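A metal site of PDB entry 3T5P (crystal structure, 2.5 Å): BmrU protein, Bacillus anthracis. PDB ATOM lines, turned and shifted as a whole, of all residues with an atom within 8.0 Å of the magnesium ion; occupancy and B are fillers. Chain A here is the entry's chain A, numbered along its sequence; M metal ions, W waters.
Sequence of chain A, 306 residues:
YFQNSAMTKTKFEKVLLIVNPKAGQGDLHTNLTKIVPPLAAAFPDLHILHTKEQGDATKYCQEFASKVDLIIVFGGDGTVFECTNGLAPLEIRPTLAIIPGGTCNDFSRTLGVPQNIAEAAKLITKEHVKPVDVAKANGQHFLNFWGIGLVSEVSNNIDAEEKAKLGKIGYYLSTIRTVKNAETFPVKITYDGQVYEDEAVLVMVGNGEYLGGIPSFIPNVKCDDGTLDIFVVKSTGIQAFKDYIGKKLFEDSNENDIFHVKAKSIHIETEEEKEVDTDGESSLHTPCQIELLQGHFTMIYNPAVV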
ATOM      1  N   ASP A 133       5.240   1.389 -12.162  1.00  0.00           N
ATOM      2  CA  ASP A 133       5.913   2.175 -11.140  1.00  0.00           C
ATOM      3  C   ASP A 133       4.985   3.264 -10.636  1.00  0.00           C
ATOM      4  O   ASP A 133       4.202   3.823 -11.415  1.00  0.00           O
ATOM      5  CB  ASP A 133       7.190   2.813 -11.666  1.00  0.00           C
ATOM      6  CG  ASP A 133       8.168   1.813 -12.215  1.00  0.00           C
ATOM      7  OD1 ASP A 133       8.072   0.635 -11.811  1.00  0.00           O
ATOM      8  OD2 ASP A 133       9.038   2.205 -13.031  1.00  0.00           O
ATOM      9  N   GLY A 206       8.687  13.110 -14.602  1.00  0.00           N
ATOM     10  CA  GLY A 206       7.712  12.317 -15.343  1.00  0.00           C
ATOM     11  C   GLY A 206       7.793  10.844 -15.002  1.00  0.00           C
ATOM     12  O   GLY A 206       8.871  10.261 -14.875  1.00  0.00           O
ATOM     13  N   ASN A 207       6.636  10.225 -14.864  1.00  0.00           N
ATOM     14  CA  ASN A 207       6.552   8.793 -14.723  1.00  0.00           C
ATOM     15  C   ASN A 207       5.862   8.145 -15.892  1.00  0.00           C
ATOM     16  O   ASN A 207       6.298   7.082 -16.366  1.00  0.00           O
ATOM     17  CB  ASN A 207       5.789   8.422 -13.434  1.00  0.00           C
ATOM     18  CG  ASN A 207       5.790   6.921 -13.185  1.00  0.00           C
ATOM     19  OD1 ASN A 207       6.848   6.332 -13.051  1.00  0.00           O
ATOM     20  ND2 ASN A 207       4.621   6.302 -13.150  1.00  0.00           N
ATOM     21  N   GLY A 208       4.776   8.770 -16.334  1.00  0.00           N
ATOM     22  CA  GLY A 208       3.948   8.234 -17.420  1.00  0.00           C
ATOM     23  C   GLY A 208       4.510   8.583 -18.774  1.00  0.00           C
ATOM     24  O   GLY A 208       5.364   9.469 -18.894  1.00  0.00           O
ATOM     25  N   GLU A 209       4.002   7.868 -19.787  1.00  0.00           N
ATOM     26  CA  GLU A 209       4.537   7.922 -21.151  1.00  0.00           C
ATOM     27  C   GLU A 209       3.729   8.849 -22.056  1.00  0.00           C
ATOM     28  O   GLU A 209       4.138   9.128 -23.208  1.00  0.00           O
ATOM     29  CB  GLU A 209       4.619   6.499 -21.727  1.00  0.00           C
ATOM     30  CG  GLU A 209       5.524   5.617 -20.900  1.00  0.00           C
ATOM     31  CD  GLU A 209       5.446   4.140 -21.227  1.00  0.00           C
ATOM     32  OE1 GLU A 209       5.149   3.790 -22.401  1.00  0.00           O
ATOM     33  OE2 GLU A 209       5.729   3.323 -20.299  1.00  0.00           O
ATOM     34  N   ASN A 220      11.877   9.368 -23.880  1.00  0.00           N
ATOM     35  CA  ASN A 220      12.208   8.019 -23.441  1.00  0.00           C
ATOM     36  C   ASN A 220      11.822   7.757 -21.979  1.00  0.00           C
ATOM     37  O   ASN A 220      12.555   7.100 -21.218  1.00  0.00           O
ATOM     38  CB  ASN A 220      13.700   7.767 -23.651  1.00  0.00           C
ATOM     39  CG  ASN A 220      14.140   8.126 -25.073  1.00  0.00           C
ATOM     40  OD1 ASN A 220      15.148   8.821 -25.259  1.00  0.00           O
ATOM     41  ND2 ASN A 220      13.363   7.680 -26.096  1.00  0.00           N
ATOM     42  N   VAL A 221      10.654   8.274 -21.597  1.00  0.00           N
ATOM     43  CA  VAL A 221      10.103   7.996 -20.301  1.00  0.00           C
ATOM     44  C   VAL A 221       9.416   6.639 -20.365  1.00  0.00           C
ATOM     45  O   VAL A 221       8.701   6.349 -21.302  1.00  0.00           O
ATOM     46  CB  VAL A 221       9.064   9.034 -19.873  1.00  0.00           C
ATOM     47  CG1 VAL A 221       8.548   8.701 -18.461  1.00  0.00           C
ATOM     48  CG2 VAL A 221       9.670  10.415 -19.877  1.00  0.00           C
ATOM     49  N   LYS A 222       9.649   5.831 -19.348  1.00  0.00           N
ATOM     50  CA  LYS A 222       8.966   4.560 -19.220  1.00  0.00           C
ATOM     51  C   LYS A 222       8.376   4.453 -17.804  1.00  0.00           C
ATOM     52  O   LYS A 222       8.999   4.861 -16.804  1.00  0.00           O
ATOM     53  CB  LYS A 222       9.926   3.401 -19.518  1.00  0.00           C
ATOM     54  CG  LYS A 222      10.430   3.374 -20.939  1.00  0.00           C
ATOM     55  CD  LYS A 222       9.297   3.234 -21.984  1.00  0.00           C
ATOM     56  CE  LYS A 222       9.873   3.467 -23.385  1.00  0.00           C
ATOM     57  NZ  LYS A 222       8.925   3.117 -24.497  1.00  0.00           N
ATOM     58  N   CYS A 223       7.157   3.912 -17.745  1.00  0.00           N
ATOM     59  CA  CYS A 223       6.397   3.842 -16.492  1.00  0.00           C
ATOM     60  C   CYS A 223       6.739   2.612 -15.681  1.00  0.00           C
ATOM     61  O   CYS A 223       6.244   2.471 -14.592  1.00  0.00           O
ATOM     62  CB  CYS A 223       4.898   3.862 -16.754  1.00  0.00           C
ATOM     63  SG  CYS A 223       4.215   2.363 -17.425  1.00  0.00           S
ATOM     64  N   ASP A 224       7.589   1.734 -16.220  1.00  0.00           N
ATOM     65  CA  ASP A 224       7.904   0.466 -15.569  1.00  0.00           C
ATOM     66  C   ASP A 224       9.388   0.110 -15.604  1.00  0.00           C
ATOM     67  O   ASP A 224       9.748  -1.050 -15.554  1.00  0.00           O
ATOM     68  CB  ASP A 224       7.096  -0.662 -16.205  1.00  0.00           C
ATOM     69  CG  ASP A 224       7.293  -0.744 -17.712  1.00  0.00           C
ATOM     70  OD1 ASP A 224       7.957   0.126 -18.297  1.00  0.00           O
ATOM     71  OD2 ASP A 224       6.764  -1.685 -18.322  1.00  0.00           O
ATOM     72  N   ASP A 225      10.243   1.114 -15.649  1.00  0.00           N
ATOM     73  CA  ASP A 225      11.689   0.905 -15.733  1.00  0.00           C
ATOM     74  C   ASP A 225      12.423   1.151 -14.415  1.00  0.00           C
ATOM     75  O   ASP A 225      13.640   1.152 -14.364  1.00  0.00           O
ATOM     76  CB  ASP A 225      12.289   1.790 -16.833  1.00  0.00           C
ATOM     77  CG  ASP A 225      12.099   3.261 -16.578  1.00  0.00           C
ATOM     78  OD1 ASP A 225      11.359   3.635 -15.632  1.00  0.00           O
ATOM     79  OD2 ASP A 225      12.676   4.049 -17.361  1.00  0.00           O
ATOM     80  N   GLY A 226      11.666   1.406 -13.357  1.00  0.00           N
ATOM     81  CA  GLY A 226      12.238   1.580 -12.026  1.00  0.00           C
ATOM     82  C   GLY A 226      12.864   2.925 -11.804  1.00  0.00           C
ATOM     83  O   GLY A 226      13.566   3.113 -10.809  1.00  0.00           O
ATOM     84  N   THR A 227      12.624   3.866 -12.698  1.00  0.00           N
ATOM     85  CA  THR A 227      13.252   5.190 -12.594  1.00  0.00           C
ATOM     86  C   THR A 227      12.378   6.322 -13.170  1.00  0.00           C
ATOM     87  O   THR A 227      11.560   6.109 -14.094  1.00  0.00           O
ATOM     88  CB  THR A 227      14.653   5.197 -13.258  1.00  0.00           C
ATOM     89  OG1 THR A 227      15.333   6.415 -12.939  1.00  0.00           O
ATOM     90  CG2 THR A 227      14.537   5.079 -14.769  1.00  0.00           C
ATOM     91  N   LEU A 228      12.561   7.522 -12.610  1.00  0.00           N
ATOM     92  CA  LEU A 228      11.789   8.702 -12.987  1.00  0.00           C
ATOM     93  C   LEU A 228      12.628   9.617 -13.868  1.00  0.00           C
ATOM     94  O   LEU A 228      13.853   9.582 -13.801  1.00  0.00           O
ATOM     95  CB  LEU A 228      11.344   9.500 -11.760  1.00  0.00           C
ATOM     96  CG  LEU A 228      10.263   8.903 -10.868  1.00  0.00           C
ATOM     97  CD1 LEU A 228      10.278   9.579  -9.529  1.00  0.00           C
ATOM     98  CD2 LEU A 228       8.884   9.005 -11.503  1.00  0.00           C
ATOM     99  N   ASP A 229      11.962  10.437 -14.675  1.00  0.00           N
ATOM    100  CA  ASP A 229      12.649  11.358 -15.574  1.00  0.00           C
ATOM    101  C   ASP A 229      12.524  12.812 -15.131  1.00  0.00           C
ATOM    102  O   ASP A 229      11.428  13.359 -15.121  1.00  0.00           O
ATOM    103  CB  ASP A 229      12.115  11.205 -16.987  1.00  0.00           C
ATOM    104  CG  ASP A 229      12.561   9.902 -17.632  1.00  0.00           C
ATOM    105  OD1 ASP A 229      13.484   9.949 -18.471  1.00  0.00           O
ATOM    106  OD2 ASP A 229      12.007   8.843 -17.246  1.00  0.00           O
ATOM    107  N   LYS A 262      17.678  10.744 -15.578  1.00  0.00           N
ATOM    108  CA  LYS A 262      16.866   9.719 -14.903  1.00  0.00           C
ATOM    109  C   LYS A 262      17.336   9.534 -13.463  1.00  0.00           C
ATOM    110  O   LYS A 262      18.525   9.571 -13.189  1.00  0.00           O
ATOM    111  CB  LYS A 262      16.921   8.382 -15.644  1.00  0.00           C
ATOM    112  CG  LYS A 262      16.280   8.421 -17.026  1.00  0.00           C
ATOM    113  CD  LYS A 262      15.854   7.023 -17.492  1.00  0.00           C
ATOM    114  CE  LYS A 262      15.538   6.941 -18.995  1.00  0.00           C
ATOM    115  NZ  LYS A 262      14.503   7.886 -19.489  1.00  0.00           N
ATOM    116  N   ALA A 263      16.376   9.339 -12.551  1.00  0.00           N
ATOM    117  CA  ALA A 263      16.683   9.187 -11.136  1.00  0.00           C
ATOM    118  C   ALA A 263      15.582   8.470 -10.371  1.00  0.00           C
ATOM    119  O   ALA A 263      14.401   8.515 -10.757  1.00  0.00           O
ATOM    120  CB  ALA A 263      16.960  10.536 -10.508  1.00  0.00           C
ATOM    121  N   LEU A 292      10.726   6.745  -6.221  1.00  0.00           N
ATOM    122  CA  LEU A 292      10.132   5.790  -7.128  1.00  0.00           C
ATOM    123  C   LEU A 292       9.915   4.455  -6.444  1.00  0.00           C
ATOM    124  O   LEU A 292      10.827   3.883  -5.879  1.00  0.00           O
ATOM    125  CB  LEU A 292      10.913   5.580  -8.420  1.00  0.00           C
ATOM    126  CG  LEU A 292       9.980   4.885  -9.427  1.00  0.00           C
ATOM    127  CD1 LEU A 292       9.048   5.887 -10.079  1.00  0.00           C
ATOM    128  CD2 LEU A 292      10.707   4.099 -10.429  1.00  0.00           C
HETATM  129 MG    MG M   1      10.329   5.323 -15.462  1.00  0.00          MG
HETATM  130  O   HOH W   1       9.275   7.041 -15.386  1.00  0.00           O
HETATM  131  O   HOH W   2      11.449   6.319 -17.134  1.00  0.00           O
HETATM  132  O   HOH W   3       8.958   4.622 -14.014  1.00  0.00           O
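The magnesium ion is bound by the backbone carbonyl oxygen of Lys 222, the side-chain carboxylate of Asp 225, the backbone carbonyl oxygen of Thr 227, water W1, water W3 and water W2.
The backbone NH of Asp 225 is in hydrogen-bond range of the side-chain carboxylate of Asp 133, 3.1 Å away.
The side-chain hydroxyl (OG1) of Thr 227 lies within hydrogen-bond range of the backbone NH (N) of Ala 263 (3.1 Å).
Water W3 bridges OD2 of Asp 133 and OD1 of Asn 207.
Water W2 lies within hydrogen-bond range of the side-chain carboxylate of Asp 229 (2.6 Å), the side-chain carboxylate of Asp 225 (2.6 Å) and the backbone NH of Lys 222 (2.9 Å).
Of the 18 residues printed, 3 come within 4 Å of the magnesium ion.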
